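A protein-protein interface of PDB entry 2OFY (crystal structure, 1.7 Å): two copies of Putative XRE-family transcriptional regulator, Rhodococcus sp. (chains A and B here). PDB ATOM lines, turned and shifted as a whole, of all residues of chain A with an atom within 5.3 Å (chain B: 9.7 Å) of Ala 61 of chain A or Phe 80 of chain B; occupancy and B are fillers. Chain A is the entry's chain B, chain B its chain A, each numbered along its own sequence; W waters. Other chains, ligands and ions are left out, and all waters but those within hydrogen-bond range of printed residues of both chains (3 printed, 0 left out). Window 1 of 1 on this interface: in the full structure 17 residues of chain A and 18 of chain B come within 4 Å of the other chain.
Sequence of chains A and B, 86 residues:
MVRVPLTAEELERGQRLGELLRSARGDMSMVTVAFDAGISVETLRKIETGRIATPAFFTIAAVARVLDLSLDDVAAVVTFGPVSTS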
ATOM      1  N   ASP A  36     -12.991  12.521 -14.227  1.00  0.00           N
ATOM      2  CA  ASP A  36     -12.003  13.604 -14.131  1.00  0.00           C
ATOM      3  C   ASP A  36     -12.199  14.426 -12.854  1.00  0.00           C
ATOM      4  O   ASP A  36     -11.239  14.983 -12.326  1.00  0.00           O
ATOM      5  CB  ASP A  36     -11.979  14.531 -15.374  1.00  0.00           C
ATOM      6  CG  ASP A  36     -11.045  14.008 -16.515  1.00  0.00           C
ATOM      7  OD1 ASP A  36     -10.594  12.848 -16.502  1.00  0.00           O
ATOM      8  OD2 ASP A  36     -10.750  14.781 -17.454  1.00  0.00           O
ATOM      9  N   ALA A  37     -13.433  14.486 -12.370  1.00  0.00           N
ATOM     10  CA  ALA A  37     -13.741  15.202 -11.129  1.00  0.00           C
ATOM     11  C   ALA A  37     -13.497  14.358  -9.862  1.00  0.00           C
ATOM     12  O   ALA A  37     -13.425  14.932  -8.763  1.00  0.00           O
ATOM     13  CB  ALA A  37     -15.140  15.629 -11.162  1.00  0.00           C
ATOM     14  N   ALA A  56     -22.166  19.306  -1.992  1.00  0.00           N
ATOM     15  CA  ALA A  56     -20.928  19.525  -1.244  1.00  0.00           C
ATOM     16  C   ALA A  56     -20.126  20.549  -2.034  1.00  0.00           C
ATOM     17  O   ALA A  56     -20.053  20.468  -3.291  1.00  0.00           O
ATOM     18  CB  ALA A  56     -20.136  18.223  -1.203  1.00  0.00           C
ATOM     19  N   PHE A  57     -19.476  21.467  -1.314  1.00  0.00           N
ATOM     20  CA  PHE A  57     -18.577  22.420  -1.954  1.00  0.00           C
ATOM     21  C   PHE A  57     -17.551  21.754  -2.860  1.00  0.00           C
ATOM     22  O   PHE A  57     -17.380  22.204  -4.027  1.00  0.00           O
ATOM     23  CB  PHE A  57     -17.781  23.226  -0.849  1.00  0.00           C
ATOM     24  CG  PHE A  57     -16.792  24.183  -1.462  1.00  0.00           C
ATOM     25  CD1 PHE A  57     -17.291  25.331  -2.152  1.00  0.00           C
ATOM     26  CD2 PHE A  57     -15.431  23.914  -1.426  1.00  0.00           C
ATOM     27  CE1 PHE A  57     -16.379  26.204  -2.807  1.00  0.00           C
ATOM     28  CE2 PHE A  57     -14.522  24.806  -2.021  1.00  0.00           C
ATOM     29  CZ  PHE A  57     -15.030  25.933  -2.715  1.00  0.00           C
ATOM     30  N   PHE A  58     -16.828  20.717  -2.371  1.00  0.00           N
ATOM     31  CA  PHE A  58     -15.749  20.132  -3.145  1.00  0.00           C
ATOM     32  C   PHE A  58     -16.265  19.340  -4.360  1.00  0.00           C
ATOM     33  O   PHE A  58     -15.559  19.181  -5.331  1.00  0.00           O
ATOM     34  CB  PHE A  58     -14.859  19.321  -2.249  1.00  0.00           C
ATOM     35  CG  PHE A  58     -13.986  20.207  -1.381  1.00  0.00           C
ATOM     36  CD1 PHE A  58     -13.099  21.110  -1.992  1.00  0.00           C
ATOM     37  CD2 PHE A  58     -14.017  20.116  -0.004  1.00  0.00           C
ATOM     38  CE1 PHE A  58     -12.231  21.904  -1.229  1.00  0.00           C
ATOM     39  CE2 PHE A  58     -13.170  20.930   0.777  1.00  0.00           C
ATOM     40  CZ  PHE A  58     -12.297  21.831   0.145  1.00  0.00           C
ATOM     41  N   THR A  59     -17.510  18.892  -4.283  1.00  0.00           N
ATOM     42  CA  THR A  59     -18.118  18.205  -5.435  1.00  0.00           C
ATOM     43  C   THR A  59     -18.354  19.217  -6.552  1.00  0.00           C
ATOM     44  O   THR A  59     -17.965  19.015  -7.698  1.00  0.00           O
ATOM     45  CB  THR A  59     -19.403  17.473  -5.061  1.00  0.00           C
ATOM     46  OG1 THR A  59     -19.054  16.450  -4.087  1.00  0.00           O
ATOM     47  CG2 THR A  59     -20.056  16.855  -6.314  1.00  0.00           C
ATOM     48  N   ILE A  60     -18.996  20.317  -6.195  1.00  0.00           N
ATOM     49  CA  ILE A  60     -19.269  21.354  -7.202  1.00  0.00           C
ATOM     50  C   ILE A  60     -17.949  21.965  -7.738  1.00  0.00           C
ATOM     51  O   ILE A  60     -17.761  22.135  -8.972  1.00  0.00           O
ATOM     52  CB  ILE A  60     -20.168  22.433  -6.586  1.00  0.00           C
ATOM     53  CG1 ILE A  60     -21.487  21.824  -6.125  1.00  0.00           C
ATOM     54  CG2 ILE A  60     -20.466  23.507  -7.667  1.00  0.00           C
ATOM     55  CD1 ILE A  60     -22.235  20.949  -7.181  1.00  0.00           C
ATOM     56  N   ALA A  61     -16.995  22.213  -6.846  1.00  0.00           N
ATOM     57  CA  ALA A  61     -15.656  22.731  -7.208  1.00  0.00           C
ATOM     58  C   ALA A  61     -14.981  21.805  -8.219  1.00  0.00           C
ATOM     59  O   ALA A  61     -14.440  22.281  -9.256  1.00  0.00           O
ATOM     60  CB  ALA A  61     -14.775  22.885  -5.957  1.00  0.00           C
ATOM     61  N   ALA A  62     -15.049  20.485  -7.982  1.00  0.00           N
ATOM     62  CA  ALA A  62     -14.386  19.509  -8.898  1.00  0.00           C
ATOM     63  C   ALA A  62     -15.040  19.501 -10.278  1.00  0.00           C
ATOM     64  O   ALA A  62     -14.338  19.517 -11.309  1.00  0.00           O
ATOM     65  CB  ALA A  62     -14.419  18.099  -8.272  1.00  0.00           C
ATOM     66  N   VAL A  63     -16.373  19.471 -10.321  1.00  0.00           N
ATOM     67  CA  VAL A  63     -17.097  19.481 -11.616  1.00  0.00           C
ATOM     68  C   VAL A  63     -16.823  20.770 -12.347  1.00  0.00           C
ATOM     69  O   VAL A  63     -16.539  20.764 -13.563  1.00  0.00           O
ATOM     70  CB  VAL A  63     -18.616  19.218 -11.408  1.00  0.00           C
ATOM     71  CG1 VAL A  63     -19.375  19.308 -12.748  1.00  0.00           C
ATOM     72  CG2 VAL A  63     -18.797  17.762 -10.772  1.00  0.00           C
ATOM     73  N   ALA A  64     -16.913  21.885 -11.607  1.00  0.00           N
ATOM     74  CA  ALA A  64     -16.624  23.192 -12.215  1.00  0.00           C
ATOM     75  C   ALA A  64     -15.231  23.169 -12.836  1.00  0.00           C
ATOM     76  O   ALA A  64     -15.046  23.703 -13.946  1.00  0.00           O
ATOM     77  CB  ALA A  64     -16.738  24.346 -11.178  1.00  0.00           C
ATOM     78  N   ARG A  65     -14.247  22.632 -12.127  1.00  0.00           N
ATOM     79  CA  ARG A  65     -12.885  22.603 -12.676  1.00  0.00           C
ATOM     80  C   ARG A  65     -12.842  21.898 -14.040  1.00  0.00           C
ATOM     81  O   ARG A  65     -12.234  22.393 -15.002  1.00  0.00           O
ATOM     82  CB  ARG A  65     -11.920  21.889 -11.708  1.00  0.00           C
ATOM     83  CG  ARG A  65     -10.479  21.988 -12.116  1.00  0.00           C
ATOM     84  CD  ARG A  65      -9.568  21.566 -10.961  1.00  0.00           C
ATOM     85  NE  ARG A  65      -9.513  22.623  -9.932  1.00  0.00           N
ATOM     86  CZ  ARG A  65      -8.673  22.651  -8.890  1.00  0.00           C
ATOM     87  NH1 ARG A  65      -7.792  21.660  -8.676  1.00  0.00           N
ATOM     88  NH2 ARG A  65      -8.730  23.672  -8.051  1.00  0.00           N
ATOM     89  N   VAL A  66     -13.424  20.702 -14.083  1.00  0.00           N
ATOM     90  CA  VAL A  66     -13.403  19.851 -15.259  1.00  0.00           C
ATOM     91  C   VAL A  66     -14.122  20.550 -16.414  1.00  0.00           C
ATOM     92  O   VAL A  66     -13.717  20.467 -17.589  1.00  0.00           O
ATOM     93  CB  VAL A  66     -14.049  18.466 -14.965  1.00  0.00           C
ATOM     94  CG1 VAL A  66     -14.177  17.616 -16.247  1.00  0.00           C
ATOM     95  CG2 VAL A  66     -13.191  17.683 -13.920  1.00  0.00           C
ATOM     96  N   LEU A  71     -16.302  29.221 -10.398  1.00  0.00           N
ATOM     97  CA  LEU A  71     -17.182  29.006  -9.228  1.00  0.00           C
ATOM     98  C   LEU A  71     -17.938  30.255  -8.783  1.00  0.00           C
ATOM     99  O   LEU A  71     -19.108  30.193  -8.324  1.00  0.00           O
ATOM    100  CB  LEU A  71     -16.389  28.454  -8.054  1.00  0.00           C
ATOM    101  CG  LEU A  71     -16.148  26.967  -8.074  1.00  0.00           C
ATOM    102  CD1 LEU A  71     -15.286  26.672  -6.834  1.00  0.00           C
ATOM    103  CD2 LEU A  71     -17.499  26.183  -8.031  1.00  0.00           C
ATOM    104  N   GLU B   9      -7.165  12.552   1.714  1.00  0.00           N
ATOM    105  CA  GLU B   9      -7.316  13.706   0.807  1.00  0.00           C
ATOM    106  C   GLU B   9      -8.530  14.598   1.138  1.00  0.00           C
ATOM    107  O   GLU B   9      -8.437  15.848   1.132  1.00  0.00           O
ATOM    108  CB  GLU B   9      -7.323  13.192  -0.645  1.00  0.00           C
ATOM    109  CG  GLU B   9      -6.020  12.474  -1.033  1.00  0.00           C
ATOM    110  CD  GLU B   9      -5.646  11.206  -0.193  1.00  0.00           C
ATOM    111  OE1 GLU B   9      -6.391  10.166  -0.161  1.00  0.00           O
ATOM    112  OE2 GLU B   9      -4.555  11.250   0.435  1.00  0.00           O
ATOM    113  N   GLU B  10      -9.667  13.992   1.453  1.00  0.00           N
ATOM    114  CA  GLU B  10     -10.838  14.750   1.859  1.00  0.00           C
ATOM    115  C   GLU B  10     -10.646  15.563   3.147  1.00  0.00           C
ATOM    116  O   GLU B  10     -11.009  16.733   3.242  1.00  0.00           O
ATOM    117  CB  GLU B  10     -12.038  13.847   1.993  1.00  0.00           C
ATOM    118  CG  GLU B  10     -12.510  13.336   0.605  1.00  0.00           C
ATOM    119  CD  GLU B  10     -13.367  12.119   0.673  1.00  0.00           C
ATOM    120  OE1 GLU B  10     -13.399  11.462   1.735  1.00  0.00           O
ATOM    121  OE2 GLU B  10     -14.019  11.802  -0.354  1.00  0.00           O
ATOM    122  N   ARG B  13      -8.268  18.452   2.433  1.00  0.00           N
ATOM    123  CA  ARG B  13      -8.935  19.563   1.711  1.00  0.00           C
ATOM    124  C   ARG B  13      -9.825  20.415   2.604  1.00  0.00           C
ATOM    125  O   ARG B  13      -9.864  21.650   2.499  1.00  0.00           O
ATOM    126  CB  ARG B  13      -9.832  19.021   0.588  1.00  0.00           C
ATOM    127  CG  ARG B  13      -9.114  18.401  -0.552  1.00  0.00           C
ATOM    128  CD  ARG B  13     -10.127  18.255  -1.705  1.00  0.00           C
ATOM    129  NE  ARG B  13      -9.578  17.415  -2.750  1.00  0.00           N
ATOM    130  CZ  ARG B  13      -9.878  16.134  -2.916  1.00  0.00           C
ATOM    131  NH1 ARG B  13     -10.750  15.523  -2.114  1.00  0.00           N
ATOM    132  NH2 ARG B  13      -9.296  15.460  -3.882  1.00  0.00           N
ATOM    133  N   GLY B  14     -10.577  19.741   3.471  1.00  0.00           N
ATOM    134  CA  GLY B  14     -11.456  20.417   4.443  1.00  0.00           C
ATOM    135  C   GLY B  14     -10.619  21.309   5.334  1.00  0.00           C
ATOM    136  O   GLY B  14     -10.973  22.447   5.624  1.00  0.00           O
ATOM    137  N   ARG B  16      -7.498  22.557   4.779  1.00  0.00           N
ATOM    138  CA  ARG B  16      -6.989  23.705   4.008  1.00  0.00           C
ATOM    139  C   ARG B  16      -8.027  24.786   3.795  1.00  0.00           C
ATOM    140  O   ARG B  16      -7.738  25.970   3.893  1.00  0.00           O
ATOM    141  CB  ARG B  16      -6.540  23.227   2.601  1.00  0.00           C
ATOM    142  CG  ARG B  16      -5.367  22.349   2.688  1.00  0.00           C
ATOM    143  CD  ARG B  16      -5.004  22.101   1.254  1.00  0.00           C
ATOM    144  NE  ARG B  16      -4.290  20.898   1.107  1.00  0.00           N
ATOM    145  CZ  ARG B  16      -4.136  20.291  -0.064  1.00  0.00           C
ATOM    146  NH1 ARG B  16      -4.684  20.814  -1.172  1.00  0.00           N
ATOM    147  NH2 ARG B  16      -3.437  19.182  -0.108  1.00  0.00           N
ATOM    148  N   LEU B  17      -9.241  24.358   3.452  1.00  0.00           N
ATOM    149  CA  LEU B  17     -10.338  25.291   3.199  1.00  0.00           C
ATOM    150  C   LEU B  17     -10.573  26.109   4.460  1.00  0.00           C
ATOM    151  O   LEU B  17     -10.699  27.333   4.410  1.00  0.00           O
ATOM    152  CB  LEU B  17     -11.599  24.511   2.782  1.00  0.00           C
ATOM    153  CG  LEU B  17     -12.850  25.388   2.633  1.00  0.00           C
ATOM    154  CD1 LEU B  17     -12.732  26.469   1.508  1.00  0.00           C
ATOM    155  CD2 LEU B  17     -14.033  24.451   2.399  1.00  0.00           C
ATOM    156  N   PRO B  55     -18.272  20.019   3.820  1.00  0.00           N
ATOM    157  CA  PRO B  55     -18.812  21.407   3.808  1.00  0.00           C
ATOM    158  C   PRO B  55     -19.742  21.654   2.610  1.00  0.00           C
ATOM    159  O   PRO B  55     -19.473  21.171   1.500  1.00  0.00           O
ATOM    160  CB  PRO B  55     -17.550  22.278   3.692  1.00  0.00           C
ATOM    161  CG  PRO B  55     -16.455  21.415   4.225  1.00  0.00           C
ATOM    162  CD  PRO B  55     -16.800  20.000   3.891  1.00  0.00           C
ATOM    163  N   ALA B  56     -20.832  22.356   2.845  1.00  0.00           N
ATOM    164  CA  ALA B  56     -21.869  22.539   1.813  1.00  0.00           C
ATOM    165  C   ALA B  56     -21.453  23.685   0.874  1.00  0.00           C
ATOM    166  O   ALA B  56     -20.941  24.714   1.324  1.00  0.00           O
ATOM    167  CB  ALA B  56     -23.240  22.865   2.458  1.00  0.00           C
ATOM    168  N   PHE B  57     -21.687  23.499  -0.434  1.00  0.00           N
ATOM    169  CA  PHE B  57     -21.311  24.519  -1.421  1.00  0.00           C
ATOM    170  C   PHE B  57     -21.916  25.880  -1.054  1.00  0.00           C
ATOM    171  O   PHE B  57     -21.214  26.918  -1.084  1.00  0.00           O
ATOM    172  CB  PHE B  57     -21.886  24.146  -2.806  1.00  0.00           C
ATOM    173  CG  PHE B  57     -21.603  25.193  -3.840  1.00  0.00           C
ATOM    174  CD1 PHE B  57     -20.300  25.383  -4.325  1.00  0.00           C
ATOM    175  CD2 PHE B  57     -22.639  26.020  -4.315  1.00  0.00           C
ATOM    176  CE1 PHE B  57     -20.045  26.405  -5.240  1.00  0.00           C
ATOM    177  CE2 PHE B  57     -22.362  27.028  -5.251  1.00  0.00           C
ATOM    178  CZ  PHE B  57     -21.071  27.218  -5.690  1.00  0.00           C
ATOM    179  N   PHE B  58     -23.209  25.886  -0.744  1.00  0.00           N
ATOM    180  CA  PHE B  58     -23.913  27.180  -0.521  1.00  0.00           C
ATOM    181  C   PHE B  58     -23.421  27.879   0.738  1.00  0.00           C
ATOM    182  O   PHE B  58     -23.297  29.101   0.744  1.00  0.00           O
ATOM    183  CB  PHE B  58     -25.417  27.014  -0.640  1.00  0.00           C
ATOM    184  CG  PHE B  58     -25.833  26.806  -2.075  1.00  0.00           C
ATOM    185  CD1 PHE B  58     -25.698  27.860  -3.008  1.00  0.00           C
ATOM    186  CD2 PHE B  58     -26.187  25.530  -2.530  1.00  0.00           C
ATOM    187  CE1 PHE B  58     -26.022  27.643  -4.331  1.00  0.00           C
ATOM    188  CE2 PHE B  58     -26.517  25.308  -3.822  1.00  0.00           C
ATOM    189  CZ  PHE B  58     -26.452  26.344  -4.743  1.00  0.00           C
ATOM    190  N   ILE B  60     -20.198  27.604   1.972  1.00  0.00           N
ATOM    191  CA  ILE B  60     -18.872  28.140   1.687  1.00  0.00           C
ATOM    192  C   ILE B  60     -19.017  29.398   0.796  1.00  0.00           C
ATOM    193  O   ILE B  60     -18.310  30.414   0.993  1.00  0.00           O
ATOM    194  CB  ILE B  60     -17.981  27.077   1.068  1.00  0.00           C
ATOM    195  CG1 ILE B  60     -17.792  25.893   2.038  1.00  0.00           C
ATOM    196  CG2 ILE B  60     -16.683  27.675   0.622  1.00  0.00           C
ATOM    197  CD1 ILE B  60     -17.260  26.267   3.448  1.00  0.00           C
ATOM    198  N   LEU B  71     -14.293  32.335  -4.819  1.00  0.00           N
ATOM    199  CA  LEU B  71     -14.327  30.853  -4.711  1.00  0.00           C
ATOM    200  C   LEU B  71     -13.298  30.208  -5.640  1.00  0.00           C
ATOM    201  O   LEU B  71     -12.797  29.146  -5.320  1.00  0.00           O
ATOM    202  CB  LEU B  71     -15.705  30.337  -5.060  1.00  0.00           C
ATOM    203  CG  LEU B  71     -16.801  30.689  -4.029  1.00  0.00           C
ATOM    204  CD1 LEU B  71     -18.187  30.239  -4.423  1.00  0.00           C
ATOM    205  CD2 LEU B  71     -16.455  30.124  -2.663  1.00  0.00           C
ATOM    206  N   ASP B  72     -13.027  30.820  -6.786  1.00  0.00           N
ATOM    207  CA  ASP B  72     -12.006  30.271  -7.699  1.00  0.00           C
ATOM    208  C   ASP B  72     -10.635  30.357  -7.080  1.00  0.00           C
ATOM    209  O   ASP B  72      -9.838  29.410  -7.230  1.00  0.00           O
ATOM    210  CB  ASP B  72     -12.049  31.003  -9.028  1.00  0.00           C
ATOM    211  CG  ASP B  72     -13.343  30.784  -9.669  1.00  0.00           C
ATOM    212  OD1 ASP B  72     -13.598  29.613 -10.054  1.00  0.00           O
ATOM    213  OD2 ASP B  72     -14.168  31.723  -9.618  1.00  0.00           O
ATOM    214  N   ASP B  73     -10.376  31.461  -6.360  1.00  0.00           N
ATOM    215  CA  ASP B  73      -9.093  31.614  -5.677  1.00  0.00           C
ATOM    216  C   ASP B  73      -8.958  30.554  -4.575  1.00  0.00           C
ATOM    217  O   ASP B  73      -7.903  29.992  -4.354  1.00  0.00           O
ATOM    218  CB  ASP B  73      -8.922  33.017  -5.111  1.00  0.00           C
ATOM    219  CG  ASP B  73      -8.730  34.092  -6.203  1.00  0.00           C
ATOM    220  OD1 ASP B  73      -8.288  33.780  -7.335  1.00  0.00           O
ATOM    221  OD2 ASP B  73      -9.035  35.278  -5.882  1.00  0.00           O
ATOM    222  N   VAL B  74     -10.058  30.267  -3.909  1.00  0.00           N
ATOM    223  CA  VAL B  74     -10.071  29.278  -2.823  1.00  0.00           C
ATOM    224  C   VAL B  74      -9.893  27.846  -3.373  1.00  0.00           C
ATOM    225  O   VAL B  74      -9.046  27.112  -2.874  1.00  0.00           O
ATOM    226  CB  VAL B  74     -11.397  29.395  -2.055  1.00  0.00           C
ATOM    227  CG1 VAL B  74     -11.686  28.152  -1.150  1.00  0.00           C
ATOM    228  CG2 VAL B  74     -11.379  30.699  -1.199  1.00  0.00           C
ATOM    229  N   ALA B  75     -10.682  27.496  -4.386  1.00  0.00           N
ATOM    230  CA  ALA B  75     -10.621  26.142  -4.978  1.00  0.00           C
ATOM    231  C   ALA B  75      -9.232  25.840  -5.539  1.00  0.00           C
ATOM    232  O   ALA B  75      -8.824  24.690  -5.558  1.00  0.00           O
ATOM    233  CB  ALA B  75     -11.672  25.979  -6.042  1.00  0.00           C
ATOM    234  N   ALA B  76      -8.507  26.880  -5.986  1.00  0.00           N
ATOM    235  CA  ALA B  76      -7.146  26.726  -6.525  1.00  0.00           C
ATOM    236  C   ALA B  76      -6.134  26.006  -5.639  1.00  0.00           C
ATOM    237  O   ALA B  76      -5.178  25.407  -6.160  1.00  0.00           O
ATOM    238  CB  ALA B  76      -6.594  28.086  -6.936  1.00  0.00           C
ATOM    239  N   VAL B  77      -6.293  26.070  -4.304  1.00  0.00           N
ATOM    240  CA  VAL B  77      -5.344  25.344  -3.418  1.00  0.00           C
ATOM    241  C   VAL B  77      -5.438  23.843  -3.378  1.00  0.00           C
ATOM    242  O   VAL B  77      -4.616  23.208  -2.725  1.00  0.00           O
ATOM    243  CB  VAL B  77      -5.362  25.835  -1.936  1.00  0.00           C
ATOM    244  CG1 VAL B  77      -5.070  27.327  -1.868  1.00  0.00           C
ATOM    245  CG2 VAL B  77      -6.682  25.451  -1.239  1.00  0.00           C
ATOM    246  N   VAL B  78      -6.478  23.269  -4.016  1.00  0.00           N
ATOM    247  CA  VAL B  78      -6.678  21.822  -4.014  1.00  0.00           C
ATOM    248  C   VAL B  78      -6.684  21.164  -5.390  1.00  0.00           C
ATOM    249  O   VAL B  78      -6.904  21.821  -6.423  1.00  0.00           O
ATOM    250  CB  VAL B  78      -7.994  21.437  -3.362  1.00  0.00           C
ATOM    251  CG1 VAL B  78      -7.953  21.714  -1.891  1.00  0.00           C
ATOM    252  CG2 VAL B  78      -9.168  22.196  -4.060  1.00  0.00           C
ATOM    253  N   THR B  79      -6.501  19.846  -5.334  1.00  0.00           N
ATOM    254  CA  THR B  79      -6.578  18.947  -6.484  1.00  0.00           C
ATOM    255  C   THR B  79      -7.772  18.011  -6.395  1.00  0.00           C
ATOM    256  O   THR B  79      -8.141  17.523  -5.312  1.00  0.00           O
ATOM    257  CB  THR B  79      -5.353  18.082  -6.589  1.00  0.00           C
ATOM    258  OG1 THR B  79      -5.262  17.227  -5.434  1.00  0.00           O
ATOM    259  CG2 THR B  79      -4.124  18.943  -6.666  1.00  0.00           C
ATOM    260  N   PHE B  80      -8.362  17.766  -7.565  1.00  0.00           N
ATOM    261  CA  PHE B  80      -9.470  16.854  -7.710  1.00  0.00           C
ATOM    262  C   PHE B  80      -9.054  15.913  -8.789  1.00  0.00           C
ATOM    263  O   PHE B  80      -8.364  16.332  -9.727  1.00  0.00           O
ATOM    264  CB  PHE B  80     -10.730  17.595  -8.172  1.00  0.00           C
ATOM    265  CG  PHE B  80     -11.051  18.827  -7.355  1.00  0.00           C
ATOM    266  CD1 PHE B  80     -11.393  18.716  -6.009  1.00  0.00           C
ATOM    267  CD2 PHE B  80     -10.994  20.079  -7.925  1.00  0.00           C
ATOM    268  CE1 PHE B  80     -11.710  19.818  -5.286  1.00  0.00           C
ATOM    269  CE2 PHE B  80     -11.298  21.156  -7.232  1.00  0.00           C
ATOM    270  CZ  PHE B  80     -11.618  21.068  -5.884  1.00  0.00           C
ATOM    271  N   GLY B  81      -9.482  14.659  -8.634  1.00  0.00           N
ATOM    272  CA  GLY B  81      -9.405  13.654  -9.674  1.00  0.00           C
ATOM    273  C   GLY B  81      -8.075  12.935  -9.634  1.00  0.00           C
ATOM    274  O   GLY B  81      -7.311  13.086  -8.662  1.00  0.00           O
ATOM    275  N   PRO B  82      -7.785  12.166 -10.697  1.00  0.00           N
ATOM    276  CA  PRO B  82      -6.542  11.425 -10.944  1.00  0.00           C
ATOM    277  C   PRO B  82      -5.325  12.352 -10.822  1.00  0.00           C
ATOM    278  O   PRO B  82      -5.253  13.391 -11.485  1.00  0.00           O
ATOM    279  CB  PRO B  82      -6.725  10.908 -12.368  1.00  0.00           C
ATOM    280  CG  PRO B  82      -8.205  10.805 -12.523  1.00  0.00           C
ATOM    281  CD  PRO B  82      -8.752  11.985 -11.793  1.00  0.00           C
ATOM    282  N   VAL B  83      -4.363  11.926 -10.007  1.00  0.00           N
ATOM    283  CA  VAL B  83      -3.488  12.840  -9.256  1.00  0.00           C
ATOM    284  C   VAL B  83      -2.352  13.668  -9.945  1.00  0.00           C
ATOM    285  O   VAL B  83      -2.153  14.818  -9.529  1.00  0.00           O
ATOM    286  CB  VAL B  83      -2.986  12.146  -7.929  1.00  0.00           C
ATOM    287  CG1 VAL B  83      -1.646  11.399  -8.122  1.00  0.00           C
ATOM    288  CG2 VAL B  83      -2.925  13.152  -6.768  1.00  0.00           C
ATOM    289  N   SER B  84      -1.634  13.194 -10.977  1.00  0.00           N
ATOM    290  CA  SER B  84      -1.973  12.104 -11.924  1.00  0.00           C
ATOM    291  C   SER B  84      -2.247  10.714 -11.291  1.00  0.00           C
ATOM    292  O   SER B  84      -2.525   9.723 -12.001  1.00  0.00           O
ATOM    293  CB  SER B  84      -0.838  12.001 -12.974  1.00  0.00           C
ATOM    294  OG  SER B  84       0.440  11.807 -12.351  1.00  0.00           O
HETATM  295  O   HOH W   1     -17.197  19.867   0.317  1.00  0.00           O
HETATM  296  O   HOH W   2      -7.027  18.605  -9.819  1.00  0.00           O
HETATM  297  O   HOH W   3     -10.445  18.112 -11.598  1.00  0.00           O
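O of Pro 55 of chain B lies within hydrogen-bond range of N of Phe 57 of chain A, 2.8 Å away. N of Leu 71 of chain A lies within hydrogen-bond range of OD1 of Asp 72 of chain B, 2.8 Å away. O of Ala 75 of chain B lies within hydrogen-bond range of NH2 of Arg 65 of chain A (2.7 Å). The backbone carbonyl oxygen of Val 78 of chain B sits at hydrogen-bond distance from the guanidinium group of Arg 65 of chain A. The backbone NH (N) of Phe 57 of chain A sits close to the backbone NH (N) of Phe 57 of chain B, 3.1 Å away.
The guanidinium group (NH2) of Arg 13 of chain B lies within hydrogen-bond range of the backbone carbonyl oxygen (O) of Thr 79 of chain B (2.8 Å).
Asp 36 of chain A touches Gly 81 of chain B. Asp 36 of chain A touches Pro 82 of chain B. Ala 37 of chain A touches Gly 81 of chain B (O to N, 3.95 Å). Phe 57 of chain B touches Ala 56 of chain A. Phe 58 of chain A touches Leu 17 of chain B. Phe 58 of chain A touches Phe 80 of chain B. CB of Ala 61 of chain A touches CZ of Phe 80 of chain B, at 3.6 Å. Arg 65 of chain A touches Ala 76 of chain B (NH2 to CA, 3.8 Å). CA of Thr 79 of chain B touches NH1 of Arg 65 of chain A, at 3.7 Å. Phe 57 of chain B touches Leu 71 of chain A.
Of chain B, only Phe 80 comes within 4 Å of Ala 61 of chain A. Of chain A, only Ala 37, Phe 58, Ala 61, Ala 62 and Arg 65 come within 4 Å of Phe 80 of chain B. Ile 60 of chain A touches just one residue of chain B: Phe 57. No residue of chain B comes within 4 Å of Ala 64 of chain A. Printed residues of chain B within 4 Å of Ala 37 of chain A: Phe 80 (3.8 Å) and Gly 81 (3.95 Å). Printed residues of chain A within 4 Å of Ala 56 of chain B: Phe 57 (3.7 Å). Printed residues of chain B within 4 Å of Phe 58 of chain A: Arg 13, Gly 14, Leu 17 and Phe 80. Printed residues of chain A within 4 Å of Ala 76 of chain B: Arg 65. Val 63 of chain A touches none of the printed residues of chain B. Thr 59 of chain A touches none of the printed residues of chain B. The nearest residue of chain A that does not touch Phe 80 of chain B is Asp 36 of chain A (4.1 Å). The nearest printed residue of chain B that does not touch Ala 56 of chain A is Ala 56 of chain B (4.4 Å).
Of the 14 printed residues of chain A, 10 touch a printed residue of chain B. Hydrophobic or aromatic side chains of chain A within 4 Å of the printed part of chain B: Phe 57, Phe 58, Ile 60, Ala 61, Ala 62 and Leu 71. Hydrophobic or aromatic side chains of chain B within 4 Å of the printed part of chain A: Leu 17, Phe 57, Ile 60, Leu 71, Ala 75, Phe 80 and Pro 82. Among the printed residues, 27 pairs touch across the chains.
Ala 56 of chain A touches Phe 57 of chain B, and with the chains exchanged Phe 57 of chain A touches Ala 56 of chain B. Phe 57 of chain B touches its own counterpart, Phe 57 of chain A. Phe 57 of chain A touches Ile 60 of chain B, and with the chains exchanged Ile 60 of chain A touches Phe 57 of chain B. Leu 71 of chain A touches its own counterpart, Leu 71 of chain B. Positions printed for both chains: 56, 57, 58, 60 and 71. Of the 27 pairs that touch across the chains among the printed residues, 8 have their exchanged pair printed and touching as well.
Water W2 bridges O of Phe 80 of chain B (2.6 Å) and NH1 of Arg 65 of chain A (3.4 Å). Water W1 lies within hydrogen-bond range of the backbone NH of Phe 58 of chain A (2.8 Å), the backbone carbonyl oxygen of Pro 55 of chain B (2.9 Å) and the backbone NH of Phe 57 of chain A (3.2 Å). Water W3 lies within hydrogen-bond range of O of Asp 36 of chain A (3.3 Å) and O of Phe 80 of chain B (3.3 Å).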
